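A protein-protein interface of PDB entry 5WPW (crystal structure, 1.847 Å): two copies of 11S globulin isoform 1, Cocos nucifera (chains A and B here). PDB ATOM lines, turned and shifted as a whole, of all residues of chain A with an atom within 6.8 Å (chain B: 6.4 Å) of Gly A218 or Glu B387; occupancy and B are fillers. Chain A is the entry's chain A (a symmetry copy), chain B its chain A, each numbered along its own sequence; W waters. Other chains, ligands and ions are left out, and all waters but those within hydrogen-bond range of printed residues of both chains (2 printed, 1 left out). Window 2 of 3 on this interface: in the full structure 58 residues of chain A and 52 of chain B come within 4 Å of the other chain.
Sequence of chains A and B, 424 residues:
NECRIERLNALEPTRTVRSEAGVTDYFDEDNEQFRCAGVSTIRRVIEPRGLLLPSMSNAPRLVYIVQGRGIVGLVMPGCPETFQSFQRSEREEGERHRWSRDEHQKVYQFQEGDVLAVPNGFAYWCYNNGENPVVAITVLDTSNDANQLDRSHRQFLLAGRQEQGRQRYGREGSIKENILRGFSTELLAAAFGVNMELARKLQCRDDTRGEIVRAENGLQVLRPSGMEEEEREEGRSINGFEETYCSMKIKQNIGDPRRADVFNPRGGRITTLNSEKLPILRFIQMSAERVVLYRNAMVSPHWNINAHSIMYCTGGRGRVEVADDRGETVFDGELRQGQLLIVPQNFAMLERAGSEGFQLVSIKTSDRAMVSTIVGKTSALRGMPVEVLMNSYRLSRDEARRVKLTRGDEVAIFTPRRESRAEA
Water W1 lies within hydrogen-bond range of OD2 of Asp A102 (2.6 Å), O of Gln A220 (2.7 Å), N of Glu B387 (3.1 Å) and N of Val B386 (3.5 Å). Water W2 lies within hydrogen-bond range of the side-chain amide nitrogen (ND2) of Asn B391 (2.6 Å) and the backbone carbonyl oxygen (O) of Gly A218 (3.0 Å).
N of Val B386 sits at hydrogen-bond distance from OD1 of Asp A102 (3.3 Å). OE2 of Glu B387 lies within hydrogen-bond range of N of Gln A220, 2.8 Å away.
Hydrophobic or aromatic side chains of chain A within 4 Å of the printed part of chain B: Leu A51, Ala A215, Leu A219 and Val A221. Of the 11 printed residues of chain B, 5 touch a printed residue of chain A. Printed residues of chain B that touch a printed residue of chain A: Pro B385, Val B386, Glu B387, Val B388 and Asn B391. Hydrophobic or aromatic side chains of chain B within 4 Å of the printed part of chain A: Pro B385, Val B386 and Val B388. Among the printed residues, 10 pairs touch across the chains. Among the printed residues, no Asp or Glu carboxylate lies within 4 Å of a Lys or Arg side-chain nitrogen of the other chain.
O of Glu B387 sits at hydrogen-bond distance from ND2 of Asn B391 (2.9 Å). The side-chain carboxylate of Glu B387 lies within salt-bridge range of the guanidinium group of Arg B397 (2.5 Å). The backbone carbonyl oxygen of Val B388 is in hydrogen-bond range of the side-chain hydroxyl of Ser B392 (2.4 Å). N of Ala A215 lies within hydrogen-bond range of O of Arg A49 (2.9 Å). The backbone NH (N) of Leu A219 is in hydrogen-bond range of the side-chain hydroxyl (OH) of Tyr A127, 3.0 Å away.
Leu A51 touches Asn B391 (CD2 to CB, 3.8 Å). Asp A102 touches Pro B385 (OD1 to CA, 3.98 Å). CA of Ala A215 touches OD1 of Asn B391, 3.6 Å away. Gly A218 touches Glu B387. Leu A219 touches Glu B387 (CD1 to O, 3.5 Å). Leu A219 touches Val B388 (CD1 to N, 3.7 Å). Leu A219 touches Asn B391. Val A221 touches Pro B385.
Of the printed residues of chain B, Leu A51 touches Asn B391 (3.8 Å). Gly A218 touches just one residue of chain B: Glu B387 (3.9 Å). Printed residues of chain B within 4 Å of Leu A219: Glu B387 (3.5 Å), Val B388 (3.7 Å) and Asn B391 (3.4 Å). Of the printed residues of chain B, Val A221 touches Pro B385. Of the printed residues of chain A, Glu B387 touches Gly A218 (3.9 Å), Leu A219 (3.5 Å) and Gln A220 (2.8 Å). The nearest residue of chain B that does not touch Gly A218 is Asn B391 (4.7 Å).
No position is printed for both chains. Of the 10 pairs that touch across the chains among the printed residues, none has its exchanged pair printed and touching as well.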
ATOM      1  N   ARG A  49      -7.184 -19.749 -32.451  1.00  0.00           N
ATOM      2  CA  ARG A  49      -6.898 -20.018 -31.044  1.00  0.00           C
ATOM      3  C   ARG A  49      -7.525 -21.321 -30.548  1.00  0.00           C
ATOM      4  O   ARG A  49      -7.548 -21.571 -29.333  1.00  0.00           O
ATOM      5  CB  ARG A  49      -7.322 -18.831 -30.154  1.00  0.00           C
ATOM      6  CG  ARG A  49      -6.214 -17.767 -29.992  1.00  0.00           C
ATOM      7  CD  ARG A  49      -5.604 -17.355 -31.323  1.00  0.00           C
ATOM      8  NE  ARG A  49      -4.613 -16.289 -31.184  1.00  0.00           N
ATOM      9  CZ  ARG A  49      -3.739 -15.943 -32.129  1.00  0.00           C
ATOM     10  NH1 ARG A  49      -3.721 -16.584 -33.295  1.00  0.00           N
ATOM     11  NH2 ARG A  49      -2.878 -14.956 -31.905  1.00  0.00           N
ATOM     12  N   LEU A  51      -7.445 -25.394 -30.087  1.00  0.00           N
ATOM     13  CA  LEU A  51      -6.504 -26.494 -29.903  1.00  0.00           C
ATOM     14  C   LEU A  51      -7.258 -27.811 -30.042  1.00  0.00           C
ATOM     15  O   LEU A  51      -8.228 -28.053 -29.317  1.00  0.00           O
ATOM     16  CB  LEU A  51      -5.825 -26.393 -28.530  1.00  0.00           C
ATOM     17  CG  LEU A  51      -5.062 -27.607 -27.992  1.00  0.00           C
ATOM     18  CD1 LEU A  51      -3.737 -27.762 -28.754  1.00  0.00           C
ATOM     19  CD2 LEU A  51      -4.831 -27.438 -26.507  1.00  0.00           C
ATOM     20  N   ASP A 102      10.360 -24.859 -20.065  1.00  0.00           N
ATOM     21  CA  ASP A 102       9.545 -25.737 -20.896  1.00  0.00           C
ATOM     22  C   ASP A 102      10.499 -26.665 -21.638  1.00  0.00           C
ATOM     23  O   ASP A 102      11.632 -26.288 -21.949  1.00  0.00           O
ATOM     24  CB  ASP A 102       8.665 -24.913 -21.867  1.00  0.00           C
ATOM     25  CG  ASP A 102       7.392 -25.659 -22.360  1.00  0.00           C
ATOM     26  OD1 ASP A 102       7.181 -26.839 -22.028  1.00  0.00           O
ATOM     27  OD2 ASP A 102       6.599 -25.048 -23.143  1.00  0.00           O
ATOM     28  N   TYR A 127      -2.845 -26.918 -33.308  1.00  0.00           N
ATOM     29  CA  TYR A 127      -3.252 -25.602 -32.802  1.00  0.00           C
ATOM     30  C   TYR A 127      -3.276 -24.575 -33.933  1.00  0.00           C
ATOM     31  O   TYR A 127      -2.306 -24.446 -34.693  1.00  0.00           O
ATOM     32  CB  TYR A 127      -2.322 -25.139 -31.681  1.00  0.00           C
ATOM     33  CG  TYR A 127      -2.563 -23.700 -31.197  1.00  0.00           C
ATOM     34  CD1 TYR A 127      -3.679 -23.378 -30.426  1.00  0.00           C
ATOM     35  CD2 TYR A 127      -1.663 -22.679 -31.508  1.00  0.00           C
ATOM     36  CE1 TYR A 127      -3.901 -22.044 -29.970  1.00  0.00           C
ATOM     37  CE2 TYR A 127      -1.874 -21.340 -31.068  1.00  0.00           C
ATOM     38  CZ  TYR A 127      -2.989 -21.040 -30.299  1.00  0.00           C
ATOM     39  OH  TYR A 127      -3.191 -19.725 -29.854  1.00  0.00           O
ATOM     40  N   ALA A 215      -8.087 -21.683 -26.525  1.00  0.00           N
ATOM     41  CA  ALA A 215      -7.010 -21.154 -25.689  1.00  0.00           C
ATOM     42  C   ALA A 215      -7.165 -19.634 -25.687  1.00  0.00           C
ATOM     43  O   ALA A 215      -6.765 -18.964 -26.640  1.00  0.00           O
ATOM     44  CB  ALA A 215      -5.638 -21.573 -26.206  1.00  0.00           C
ATOM     45  N   GLU A 216      -7.747 -19.087 -24.617  1.00  0.00           N
ATOM     46  CA  GLU A 216      -8.090 -17.663 -24.641  1.00  0.00           C
ATOM     47  C   GLU A 216      -6.862 -16.767 -24.486  1.00  0.00           C
ATOM     48  O   GLU A 216      -6.872 -15.625 -24.957  1.00  0.00           O
ATOM     49  CB  GLU A 216      -9.126 -17.338 -23.560  1.00  0.00           C
ATOM     50  CG  GLU A 216      -9.914 -16.056 -23.851  1.00  0.00           C
ATOM     51  CD  GLU A 216     -11.235 -15.978 -23.096  1.00  0.00           C
ATOM     52  OE1 GLU A 216     -11.243 -15.464 -21.954  1.00  0.00           O
ATOM     53  OE2 GLU A 216     -12.265 -16.423 -23.648  1.00  0.00           O
ATOM     54  N   ASN A 217      -5.798 -17.258 -23.845  1.00  0.00           N
ATOM     55  CA  ASN A 217      -4.555 -16.509 -23.719  1.00  0.00           C
ATOM     56  C   ASN A 217      -3.576 -16.778 -24.844  1.00  0.00           C
ATOM     57  O   ASN A 217      -2.399 -16.414 -24.727  1.00  0.00           O
ATOM     58  CB  ASN A 217      -3.877 -16.830 -22.389  1.00  0.00           C
ATOM     59  CG  ASN A 217      -4.489 -16.089 -21.249  1.00  0.00           C
ATOM     60  OD1 ASN A 217      -4.922 -14.945 -21.408  1.00  0.00           O
ATOM     61  ND2 ASN A 217      -4.538 -16.726 -20.078  1.00  0.00           N
ATOM     62  N   GLY A 218      -4.018 -17.422 -25.915  1.00  0.00           N
ATOM     63  CA  GLY A 218      -3.096 -17.885 -26.926  1.00  0.00           C
ATOM     64  C   GLY A 218      -2.384 -19.105 -26.392  1.00  0.00           C
ATOM     65  O   GLY A 218      -2.413 -19.378 -25.187  1.00  0.00           O
ATOM     66  N   LEU A 219      -1.758 -19.871 -27.259  1.00  0.00           N
ATOM     67  CA  LEU A 219      -0.986 -21.027 -26.832  1.00  0.00           C
ATOM     68  C   LEU A 219       0.467 -20.720 -27.130  1.00  0.00           C
ATOM     69  O   LEU A 219       0.845 -20.576 -28.293  1.00  0.00           O
ATOM     70  CB  LEU A 219      -1.441 -22.292 -27.554  1.00  0.00           C
ATOM     71  CG  LEU A 219      -0.753 -23.573 -27.096  1.00  0.00           C
ATOM     72  CD1 LEU A 219      -1.445 -24.057 -25.854  1.00  0.00           C
ATOM     73  CD2 LEU A 219      -0.792 -24.638 -28.195  1.00  0.00           C
ATOM     74  N   GLN A 220       1.288 -20.626 -26.096  1.00  0.00           N
ATOM     75  CA  GLN A 220       2.712 -20.413 -26.293  1.00  0.00           C
ATOM     76  C   GLN A 220       3.432 -21.742 -26.132  1.00  0.00           C
ATOM     77  O   GLN A 220       3.283 -22.420 -25.110  1.00  0.00           O
ATOM     78  CB  GLN A 220       3.276 -19.377 -25.324  1.00  0.00           C
ATOM     79  CG  GLN A 220       2.784 -17.958 -25.606  1.00  0.00           C
ATOM     80  CD  GLN A 220       3.676 -17.205 -26.581  1.00  0.00           C
ATOM     81  OE1 GLN A 220       3.292 -16.958 -27.726  1.00  0.00           O
ATOM     82  NE2 GLN A 220       4.875 -16.843 -26.132  1.00  0.00           N
ATOM     83  N   VAL A 221       4.187 -22.114 -27.156  1.00  0.00           N
ATOM     84  CA  VAL A 221       5.055 -23.279 -27.127  1.00  0.00           C
ATOM     85  C   VAL A 221       6.415 -22.815 -27.617  1.00  0.00           C
ATOM     86  O   VAL A 221       6.557 -21.725 -28.167  1.00  0.00           O
ATOM     87  CB  VAL A 221       4.521 -24.431 -28.002  1.00  0.00           C
ATOM     88  CG1 VAL A 221       3.076 -24.729 -27.684  1.00  0.00           C
ATOM     89  CG2 VAL A 221       4.692 -24.098 -29.476  1.00  0.00           C
ATOM     90  N   MET B 384       4.892 -33.179 -24.600  1.00  0.00           N
ATOM     91  CA  MET B 384       3.935 -32.147 -24.961  1.00  0.00           C
ATOM     92  C   MET B 384       4.250 -30.841 -24.242  1.00  0.00           C
ATOM     93  O   MET B 384       4.700 -30.848 -23.089  1.00  0.00           O
ATOM     94  CB  MET B 384       2.514 -32.597 -24.609  1.00  0.00           C
ATOM     95  CG  MET B 384       1.884 -33.460 -25.717  1.00  0.00           C
ATOM     96  SD  MET B 384       0.301 -34.095 -25.179  1.00  0.00           S
ATOM     97  CE  MET B 384       0.359 -35.664 -26.111  1.00  0.00           C
ATOM     98  N   PRO B 385       4.045 -29.707 -24.912  1.00  0.00           N
ATOM     99  CA  PRO B 385       4.283 -28.411 -24.257  1.00  0.00           C
ATOM    100  C   PRO B 385       3.395 -28.235 -23.032  1.00  0.00           C
ATOM    101  O   PRO B 385       2.220 -28.615 -23.032  1.00  0.00           O
ATOM    102  CB  PRO B 385       3.936 -27.396 -25.349  1.00  0.00           C
ATOM    103  CG  PRO B 385       4.108 -28.166 -26.659  1.00  0.00           C
ATOM    104  CD  PRO B 385       3.682 -29.564 -26.337  1.00  0.00           C
ATOM    105  N   VAL B 386       3.957 -27.613 -21.990  1.00  0.00           N
ATOM    106  CA  VAL B 386       3.167 -27.382 -20.778  1.00  0.00           C
ATOM    107  C   VAL B 386       1.823 -26.744 -21.117  1.00  0.00           C
ATOM    108  O   VAL B 386       0.787 -27.122 -20.556  1.00  0.00           O
ATOM    109  CB  VAL B 386       3.958 -26.541 -19.757  1.00  0.00           C
ATOM    110  CG1 VAL B 386       5.229 -27.253 -19.363  1.00  0.00           C
ATOM    111  CG2 VAL B 386       4.271 -25.166 -20.314  1.00  0.00           C
ATOM    112  N   GLU B 387       1.796 -25.799 -22.074  1.00  0.00           N
ATOM    113  CA  GLU B 387       0.559 -25.055 -22.300  1.00  0.00           C
ATOM    114  C   GLU B 387      -0.476 -25.891 -23.023  1.00  0.00           C
ATOM    115  O   GLU B 387      -1.676 -25.689 -22.820  1.00  0.00           O
ATOM    116  CB  GLU B 387       0.825 -23.746 -23.058  1.00  0.00           C
ATOM    117  CG  GLU B 387       1.745 -22.785 -22.281  1.00  0.00           C
ATOM    118  CD  GLU B 387       1.411 -21.297 -22.458  1.00  0.00           C
ATOM    119  OE1 GLU B 387       1.918 -20.501 -21.646  1.00  0.00           O
ATOM    120  OE2 GLU B 387       0.668 -20.918 -23.391  1.00  0.00           O
ATOM    121  N   VAL B 388      -0.039 -26.849 -23.851  1.00  0.00           N
ATOM    122  CA  VAL B 388      -0.964 -27.833 -24.395  1.00  0.00           C
ATOM    123  C   VAL B 388      -1.619 -28.625 -23.270  1.00  0.00           C
ATOM    124  O   VAL B 388      -2.833 -28.868 -23.285  1.00  0.00           O
ATOM    125  CB  VAL B 388      -0.228 -28.753 -25.390  1.00  0.00           C
ATOM    126  CG1 VAL B 388      -1.091 -29.967 -25.749  1.00  0.00           C
ATOM    127  CG2 VAL B 388       0.210 -27.965 -26.623  1.00  0.00           C
ATOM    128  N   LEU B 389      -0.832 -29.047 -22.279  1.00  0.00           N
ATOM    129  CA  LEU B 389      -1.403 -29.766 -21.143  1.00  0.00           C
ATOM    130  C   LEU B 389      -2.296 -28.860 -20.299  1.00  0.00           C
ATOM    131  O   LEU B 389      -3.352 -29.290 -19.816  1.00  0.00           O
ATOM    132  CB  LEU B 389      -0.295 -30.342 -20.271  1.00  0.00           C
ATOM    133  CG  LEU B 389       0.683 -31.365 -20.867  1.00  0.00           C
ATOM    134  CD1 LEU B 389       1.767 -31.662 -19.887  1.00  0.00           C
ATOM    135  CD2 LEU B 389      -0.023 -32.621 -21.254  1.00  0.00           C
ATOM    136  N   MET B 390      -1.869 -27.619 -20.074  1.00  0.00           N
ATOM    137  CA  MET B 390      -2.732 -26.688 -19.344  1.00  0.00           C
ATOM    138  C   MET B 390      -4.104 -26.626 -19.987  1.00  0.00           C
ATOM    139  O   MET B 390      -5.108 -27.001 -19.373  1.00  0.00           O
ATOM    140  CB  MET B 390      -2.088 -25.306 -19.286  1.00  0.00           C
ATOM    141  CG  MET B 390      -0.937 -25.250 -18.283  1.00  0.00           C
ATOM    142  SD  MET B 390       0.060 -23.759 -18.405  1.00  0.00           S
ATOM    143  CE  MET B 390      -1.161 -22.516 -17.903  1.00  0.00           C
ATOM    144  N   ASN B 391      -4.153 -26.256 -21.276  1.00  0.00           N
ATOM    145  CA  ASN B 391      -5.437 -26.102 -21.946  1.00  0.00           C
ATOM    146  C   ASN B 391      -6.180 -27.420 -22.096  1.00  0.00           C
ATOM    147  O   ASN B 391      -7.415 -27.419 -22.096  1.00  0.00           O
ATOM    148  CB  ASN B 391      -5.237 -25.421 -23.307  1.00  0.00           C
ATOM    149  CG  ASN B 391      -4.891 -23.922 -23.176  1.00  0.00           C
ATOM    150  OD1 ASN B 391      -5.774 -23.092 -22.967  1.00  0.00           O
ATOM    151  ND2 ASN B 391      -3.607 -23.581 -23.326  1.00  0.00           N
ATOM    152  N   SER B 392      -5.457 -28.560 -22.187  1.00  0.00           N
ATOM    153  CA  SER B 392      -6.106 -29.858 -22.389  1.00  0.00           C
ATOM    154  C   SER B 392      -6.870 -30.316 -21.155  1.00  0.00           C
ATOM    155  O   SER B 392      -7.980 -30.856 -21.262  1.00  0.00           O
ATOM    156  CB  SER B 392      -5.067 -30.932 -22.758  1.00  0.00           C
ATOM    157  OG  SER B 392      -4.373 -30.599 -23.965  1.00  0.00           O
ATOM    158  N   ARG B 397      -0.323 -23.897 -14.670  1.00  0.00           N
ATOM    159  CA  ARG B 397       1.047 -24.240 -15.047  1.00  0.00           C
ATOM    160  C   ARG B 397       1.714 -25.136 -13.999  1.00  0.00           C
ATOM    161  O   ARG B 397       2.409 -26.097 -14.352  1.00  0.00           O
ATOM    162  CB  ARG B 397       1.857 -22.960 -15.292  1.00  0.00           C
ATOM    163  CG  ARG B 397       3.288 -23.174 -15.734  1.00  0.00           C
ATOM    164  CD  ARG B 397       3.933 -21.879 -16.203  1.00  0.00           C
ATOM    165  NE  ARG B 397       3.543 -21.514 -17.558  1.00  0.00           N
ATOM    166  CZ  ARG B 397       2.529 -20.707 -17.850  1.00  0.00           C
ATOM    167  NH1 ARG B 397       2.246 -20.417 -19.119  1.00  0.00           N
ATOM    168  NH2 ARG B 397       1.803 -20.178 -16.870  1.00  0.00           N
ATOM    169  N   ALA B 400       0.177 -28.607 -14.345  1.00  0.00           N
ATOM    170  CA  ALA B 400       0.759 -29.153 -15.577  1.00  0.00           C
ATOM    171  C   ALA B 400       2.176 -29.671 -15.349  1.00  0.00           C
ATOM    172  O   ALA B 400       2.507 -30.804 -15.725  1.00  0.00           O
ATOM    173  CB  ALA B 400       0.760 -28.088 -16.676  1.00  0.00           C
HETATM  174  O   HOH W   1       4.098 -24.595 -23.677  1.00  0.00           O
HETATM  175  O   HOH W   2      -2.798 -21.150 -22.800  1.00  0.00           O
